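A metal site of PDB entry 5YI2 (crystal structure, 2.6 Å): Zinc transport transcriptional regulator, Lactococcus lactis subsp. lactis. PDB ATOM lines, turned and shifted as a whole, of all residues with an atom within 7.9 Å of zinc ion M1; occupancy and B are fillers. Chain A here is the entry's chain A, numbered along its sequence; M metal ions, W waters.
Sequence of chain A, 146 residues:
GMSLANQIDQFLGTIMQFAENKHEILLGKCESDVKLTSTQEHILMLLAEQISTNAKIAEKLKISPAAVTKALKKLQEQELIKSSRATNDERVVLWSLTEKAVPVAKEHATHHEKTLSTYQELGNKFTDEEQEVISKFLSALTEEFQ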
ATOM      1  N   LEU A  26     -22.551 -24.213 -15.322  1.00  0.00           N
ATOM      2  CA  LEU A  26     -23.131 -25.169 -14.376  1.00  0.00           C
ATOM      3  C   LEU A  26     -24.243 -24.521 -13.570  1.00  0.00           C
ATOM      4  O   LEU A  26     -24.123 -23.366 -13.154  1.00  0.00           O
ATOM      5  CB  LEU A  26     -22.058 -25.687 -13.411  1.00  0.00           C
ATOM      6  CG  LEU A  26     -20.899 -26.488 -13.989  1.00  0.00           C
ATOM      7  CD1 LEU A  26     -19.790 -26.650 -12.952  1.00  0.00           C
ATOM      8  CD2 LEU A  26     -21.393 -27.844 -14.501  1.00  0.00           C
ATOM      9  N   LYS A  29     -25.438 -24.092  -6.923  1.00  0.00           N
ATOM     10  CA  LYS A  29     -24.238 -23.671  -6.217  1.00  0.00           C
ATOM     11  C   LYS A  29     -23.137 -24.736  -6.276  1.00  0.00           C
ATOM     12  O   LYS A  29     -23.418 -25.934  -6.321  1.00  0.00           O
ATOM     13  CB  LYS A  29     -24.594 -23.333  -4.758  1.00  0.00           C
ATOM     14  CG  LYS A  29     -23.490 -22.623  -3.980  1.00  0.00           C
ATOM     15  CD  LYS A  29     -23.926 -22.258  -2.555  1.00  0.00           C
ATOM     16  CE  LYS A  29     -22.771 -21.599  -1.781  1.00  0.00           C
ATOM     17  NZ  LYS A  29     -23.150 -21.180  -0.396  1.00  0.00           N
ATOM     18  N   CYS A  30     -21.880 -24.283  -6.319  1.00  0.00           N
ATOM     19  CA  CYS A  30     -20.753 -25.182  -6.154  1.00  0.00           C
ATOM     20  C   CYS A  30     -20.617 -25.576  -4.686  1.00  0.00           C
ATOM     21  O   CYS A  30     -20.101 -24.812  -3.860  1.00  0.00           O
ATOM     22  CB  CYS A  30     -19.448 -24.550  -6.624  1.00  0.00           C
ATOM     23  SG  CYS A  30     -17.967 -25.444  -6.091  1.00  0.00           S
ATOM     24  N   GLU A  31     -21.088 -26.780  -4.378  1.00  0.00           N
ATOM     25  CA  GLU A  31     -21.130 -27.269  -3.005  1.00  0.00           C
ATOM     26  C   GLU A  31     -19.774 -27.783  -2.478  1.00  0.00           C
ATOM     27  O   GLU A  31     -19.721 -28.512  -1.488  1.00  0.00           O
ATOM     28  CB  GLU A  31     -22.204 -28.352  -2.866  1.00  0.00           C
ATOM     29  CG  GLU A  31     -23.619 -27.860  -3.173  1.00  0.00           C
ATOM     30  CD  GLU A  31     -24.639 -28.993  -3.232  1.00  0.00           C
ATOM     31  OE1 GLU A  31     -25.740 -28.779  -3.786  1.00  0.00           O
ATOM     32  OE2 GLU A  31     -24.354 -30.104  -2.714  1.00  0.00           O
ATOM     33  N   SER A  32     -18.678 -27.408  -3.133  1.00  0.00           N
ATOM     34  CA  SER A  32     -17.358 -27.781  -2.633  1.00  0.00           C
ATOM     35  C   SER A  32     -16.870 -26.877  -1.497  1.00  0.00           C
ATOM     36  O   SER A  32     -16.954 -25.644  -1.600  1.00  0.00           O
ATOM     37  CB  SER A  32     -16.328 -27.804  -3.777  1.00  0.00           C
ATOM     38  OG  SER A  32     -16.242 -29.090  -4.358  1.00  0.00           O
ATOM     39  N   ASP A  33     -16.353 -27.492  -0.436  1.00  0.00           N
ATOM     40  CA  ASP A  33     -15.823 -26.770   0.720  1.00  0.00           C
ATOM     41  C   ASP A  33     -14.650 -25.865   0.359  1.00  0.00           C
ATOM     42  O   ASP A  33     -14.366 -24.909   1.069  1.00  0.00           O
ATOM     43  CB  ASP A  33     -15.428 -27.740   1.820  1.00  0.00           C
ATOM     44  N   VAL A  34     -13.953 -26.175  -0.740  1.00  0.00           N
ATOM     45  CA  VAL A  34     -12.835 -25.328  -1.152  1.00  0.00           C
ATOM     46  C   VAL A  34     -13.260 -24.314  -2.202  1.00  0.00           C
ATOM     47  O   VAL A  34     -14.133 -24.604  -3.042  1.00  0.00           O
ATOM     48  CB  VAL A  34     -11.665 -26.143  -1.712  1.00  0.00           C
ATOM     49  CG1 VAL A  34     -10.428 -25.267  -1.784  1.00  0.00           C
ATOM     50  CG2 VAL A  34     -11.415 -27.359  -0.842  1.00  0.00           C
ATOM     51  N   LEU A  36     -12.699 -22.806  -5.441  1.00  0.00           N
ATOM     52  CA  LEU A  36     -11.961 -22.972  -6.683  1.00  0.00           C
ATOM     53  C   LEU A  36     -12.798 -22.545  -7.891  1.00  0.00           C
ATOM     54  O   LEU A  36     -14.032 -22.665  -7.885  1.00  0.00           O
ATOM     55  CB  LEU A  36     -11.515 -24.430  -6.850  1.00  0.00           C
ATOM     56  CG  LEU A  36     -10.562 -25.032  -5.811  1.00  0.00           C
ATOM     57  CD1 LEU A  36     -10.445 -26.528  -6.033  1.00  0.00           C
ATOM     58  CD2 LEU A  36      -9.206 -24.371  -5.887  1.00  0.00           C
ATOM     59  N   THR A  37     -12.122 -22.041  -8.911  1.00  0.00           N
ATOM     60  CA  THR A  37     -12.771 -21.767 -10.179  1.00  0.00           C
ATOM     61  C   THR A  37     -13.284 -23.086 -10.749  1.00  0.00           C
ATOM     62  O   THR A  37     -12.780 -24.157 -10.396  1.00  0.00           O
ATOM     63  CB  THR A  37     -11.775 -21.209 -11.207  1.00  0.00           C
ATOM     64  OG1 THR A  37     -10.727 -22.155 -11.394  1.00  0.00           O
ATOM     65  CG2 THR A  37     -11.187 -19.899 -10.733  1.00  0.00           C
ATOM     66  N   SER A  38     -14.277 -23.006 -11.627  1.00  0.00           N
ATOM     67  CA  SER A  38     -14.797 -24.229 -12.250  1.00  0.00           C
ATOM     68  C   SER A  38     -13.713 -24.889 -13.094  1.00  0.00           C
ATOM     69  O   SER A  38     -13.661 -26.116 -13.181  1.00  0.00           O
ATOM     70  CB  SER A  38     -16.039 -23.932 -13.082  1.00  0.00           C
ATOM     71  OG  SER A  38     -15.744 -23.039 -14.149  1.00  0.00           O
ATOM     72  N   GLU A  41     -11.477 -26.898 -10.646  1.00  0.00           N
ATOM     73  CA  GLU A  41     -12.199 -28.065 -10.171  1.00  0.00           C
ATOM     74  C   GLU A  41     -12.337 -29.096 -11.290  1.00  0.00           C
ATOM     75  O   GLU A  41     -12.203 -30.304 -11.080  1.00  0.00           O
ATOM     76  CB  GLU A  41     -13.570 -27.671  -9.624  1.00  0.00           C
ATOM     77  CG  GLU A  41     -13.524 -26.920  -8.303  1.00  0.00           C
ATOM     78  CD  GLU A  41     -14.833 -26.997  -7.551  1.00  0.00           C
ATOM     79  OE1 GLU A  41     -15.790 -27.585  -8.069  1.00  0.00           O
ATOM     80  OE2 GLU A  41     -14.909 -26.457  -6.426  1.00  0.00           O
ATOM     81  N   HIS A  42     -12.594 -28.603 -12.486  1.00  0.00           N
ATOM     82  CA  HIS A  42     -12.745 -29.487 -13.630  1.00  0.00           C
ATOM     83  C   HIS A  42     -11.443 -30.219 -13.937  1.00  0.00           C
ATOM     84  O   HIS A  42     -11.442 -31.365 -14.377  1.00  0.00           O
ATOM     85  CB  HIS A  42     -13.242 -28.705 -14.847  1.00  0.00           C
ATOM     86  CG  HIS A  42     -13.764 -29.564 -15.947  1.00  0.00           C
ATOM     87  ND1 HIS A  42     -15.103 -29.678 -16.229  1.00  0.00           N
ATOM     88  CD2 HIS A  42     -13.126 -30.375 -16.826  1.00  0.00           C
ATOM     89  CE1 HIS A  42     -15.274 -30.515 -17.238  1.00  0.00           C
ATOM     90  NE2 HIS A  42     -14.085 -30.947 -17.621  1.00  0.00           N
ATOM     91  N   PRO A 103     -12.528 -35.813  -2.935  1.00  0.00           N
ATOM     92  CA  PRO A 103     -13.943 -35.400  -2.757  1.00  0.00           C
ATOM     93  C   PRO A 103     -14.334 -34.180  -3.603  1.00  0.00           C
ATOM     94  O   PRO A 103     -15.423 -34.170  -4.176  1.00  0.00           O
ATOM     95  CB  PRO A 103     -14.020 -35.065  -1.257  1.00  0.00           C
ATOM     96  CG  PRO A 103     -12.604 -34.820  -0.834  1.00  0.00           C
ATOM     97  CD  PRO A 103     -11.760 -35.721  -1.675  1.00  0.00           C
ATOM     98  N   VAL A 104     -13.473 -33.172  -3.684  1.00  0.00           N
ATOM     99  CA  VAL A 104     -13.729 -32.008  -4.521  1.00  0.00           C
ATOM    100  C   VAL A 104     -13.933 -32.438  -5.956  1.00  0.00           C
ATOM    101  O   VAL A 104     -14.812 -31.941  -6.651  1.00  0.00           O
ATOM    102  CB  VAL A 104     -12.567 -30.993  -4.470  1.00  0.00           C
ATOM    103  CG1 VAL A 104     -12.858 -29.816  -5.406  1.00  0.00           C
ATOM    104  CG2 VAL A 104     -12.326 -30.487  -3.052  1.00  0.00           C
ATOM    105  N   ALA A 105     -13.108 -33.369  -6.405  1.00  0.00           N
ATOM    106  CA  ALA A 105     -13.222 -33.902  -7.750  1.00  0.00           C
ATOM    107  C   ALA A 105     -14.583 -34.557  -7.952  1.00  0.00           C
ATOM    108  O   ALA A 105     -15.247 -34.355  -8.972  1.00  0.00           O
ATOM    109  CB  ALA A 105     -12.104 -34.907  -8.021  1.00  0.00           C
ATOM    110  N   LYS A 106     -14.975 -35.355  -6.966  1.00  0.00           N
ATOM    111  CA  LYS A 106     -16.256 -36.037  -6.949  1.00  0.00           C
ATOM    112  C   LYS A 106     -17.420 -35.037  -6.968  1.00  0.00           C
ATOM    113  O   LYS A 106     -18.375 -35.205  -7.721  1.00  0.00           O
ATOM    114  CB  LYS A 106     -16.336 -36.938  -5.728  1.00  0.00           C
ATOM    115  CG  LYS A 106     -17.689 -37.597  -5.512  1.00  0.00           C
ATOM    116  CD  LYS A 106     -17.885 -38.706  -6.499  1.00  0.00           C
ATOM    117  CE  LYS A 106     -19.295 -39.266  -6.412  1.00  0.00           C
ATOM    118  NZ  LYS A 106     -19.478 -40.356  -7.415  1.00  0.00           N
ATOM    119  N   GLU A 107     -17.343 -33.989  -6.147  1.00  0.00           N
ATOM    120  CA  GLU A 107     -18.389 -32.974  -6.100  1.00  0.00           C
ATOM    121  C   GLU A 107     -18.557 -32.314  -7.472  1.00  0.00           C
ATOM    122  O   GLU A 107     -19.669 -32.164  -7.949  1.00  0.00           O
ATOM    123  CB  GLU A 107     -18.111 -31.936  -5.018  1.00  0.00           C
ATOM    124  CG  GLU A 107     -19.216 -30.879  -4.811  1.00  0.00           C
ATOM    125  CD  GLU A 107     -19.261 -29.819  -5.915  1.00  0.00           C
ATOM    126  OE1 GLU A 107     -18.217 -29.598  -6.558  1.00  0.00           O
ATOM    127  OE2 GLU A 107     -20.335 -29.211  -6.140  1.00  0.00           O
ATOM    128  N   HIS A 108     -17.449 -31.922  -8.098  1.00  0.00           N
ATOM    129  CA  HIS A 108     -17.515 -31.315  -9.422  1.00  0.00           C
ATOM    130  C   HIS A 108     -18.201 -32.230 -10.439  1.00  0.00           C
ATOM    131  O   HIS A 108     -19.043 -31.776 -11.215  1.00  0.00           O
ATOM    132  CB  HIS A 108     -16.128 -30.880  -9.907  1.00  0.00           C
ATOM    133  CG  HIS A 108     -16.167 -29.950 -11.093  1.00  0.00           C
ATOM    134  ND1 HIS A 108     -16.741 -28.696 -11.046  1.00  0.00           N
ATOM    135  CD2 HIS A 108     -15.701 -30.095 -12.362  1.00  0.00           C
ATOM    136  CE1 HIS A 108     -16.625 -28.110 -12.222  1.00  0.00           C
ATOM    137  NE2 HIS A 108     -15.994 -28.943 -13.036  1.00  0.00           N
ATOM    138  N   ALA A 109     -17.862 -33.514 -10.456  1.00  0.00           N
ATOM    139  CA  ALA A 109     -18.532 -34.459 -11.348  1.00  0.00           C
ATOM    140  C   ALA A 109     -20.042 -34.511 -11.098  1.00  0.00           C
ATOM    141  O   ALA A 109     -20.845 -34.666 -12.031  1.00  0.00           O
ATOM    142  CB  ALA A 109     -17.945 -35.848 -11.221  1.00  0.00           C
ATOM    143  N   THR A 110     -20.404 -34.375  -9.828  1.00  0.00           N
ATOM    144  CA  THR A 110     -21.789 -34.449  -9.416  1.00  0.00           C
ATOM    145  C   THR A 110     -22.522 -33.197  -9.893  1.00  0.00           C
ATOM    146  O   THR A 110     -23.619 -33.278 -10.466  1.00  0.00           O
ATOM    147  CB  THR A 110     -21.879 -34.601  -7.890  1.00  0.00           C
ATOM    148  OG1 THR A 110     -21.027 -35.668  -7.470  1.00  0.00           O
ATOM    149  CG2 THR A 110     -23.307 -34.923  -7.457  1.00  0.00           C
ATOM    150  N   HIS A 111     -21.898 -32.050  -9.689  1.00  0.00           N
ATOM    151  CA  HIS A 111     -22.425 -30.786 -10.154  1.00  0.00           C
ATOM    152  C   HIS A 111     -22.783 -30.859 -11.634  1.00  0.00           C
ATOM    153  O   HIS A 111     -23.865 -30.433 -12.038  1.00  0.00           O
ATOM    154  CB  HIS A 111     -21.403 -29.674  -9.922  1.00  0.00           C
ATOM    155  CG  HIS A 111     -22.003 -28.313  -9.871  1.00  0.00           C
ATOM    156  ND1 HIS A 111     -21.327 -27.213  -9.384  1.00  0.00           N
ATOM    157  CD2 HIS A 111     -23.228 -27.863 -10.241  1.00  0.00           C
ATOM    158  CE1 HIS A 111     -22.100 -26.150  -9.450  1.00  0.00           C
ATOM    159  NE2 HIS A 111     -23.261 -26.517  -9.977  1.00  0.00           N
ATOM    160  N   HIS A 112     -21.876 -31.408 -12.432  1.00  0.00           N
ATOM    161  CA  HIS A 112     -22.145 -31.623 -13.856  1.00  0.00           C
ATOM    162  C   HIS A 112     -23.339 -32.552 -14.066  1.00  0.00           C
ATOM    163  O   HIS A 112     -24.168 -32.299 -14.941  1.00  0.00           O
ATOM    164  CB  HIS A 112     -20.925 -32.226 -14.546  1.00  0.00           C
ATOM    165  CG  HIS A 112     -19.986 -31.205 -15.112  1.00  0.00           C
ATOM    166  ND1 HIS A 112     -20.150 -30.645 -16.362  1.00  0.00           N
ATOM    167  CD2 HIS A 112     -18.842 -30.671 -14.613  1.00  0.00           C
ATOM    168  CE1 HIS A 112     -19.163 -29.805 -16.607  1.00  0.00           C
ATOM    169  NE2 HIS A 112     -18.352 -29.800 -15.559  1.00  0.00           N
HETATM  170 ZN    ZN M   1     -17.851 -27.683  -7.380  1.00  0.00          ZN
HETATM  171 ZN    ZN M   2     -16.609 -28.744 -15.072  1.00  0.00          ZN
HETATM  172  O   HOH W   1     -17.524 -25.416  -9.958  1.00  0.00           O
HETATM  173  O   HOH W   2     -18.972 -27.135  -9.072  1.00  0.00           O
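Water W2 binds zinc ion M1 (2.1 Å). Zinc ion M1 is bound by OE1 of Glu 107. Zinc ion M1 is bound by OE1 of Glu 41 (2.2 Å). Zinc ion M1 is bound by the side-chain sulfur (SG) of Cys 30 (2.6 Å). Zinc ion M1 has four donor atoms within binding distance.
Residues that only touch zinc ion M1: Ser 32 (3.7 Å) and His 108 (3.96 Å). Of the 22 residues printed, 5 come within 4 Å of zinc ion M1. The nearest printed residue that does not touch zinc ion M1 is His 111 (4.04 Å).
OE1 of Glu 107 lies close to OG of Ser 32 (3.0 Å). The backbone NH (N) of Glu 31 lies within hydrogen-bond range of the side-chain carboxylate (OE2) of Glu 107, 3.1 Å away. The side-chain carboxylate (OE1) of Glu 41 sits close to a ring nitrogen (ND1) of His 108 (3.3 Å). The side-chain sulfur (SG) of Cys 30 lies close to the backbone NH (N) of Ser 32 (3.6 Å).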
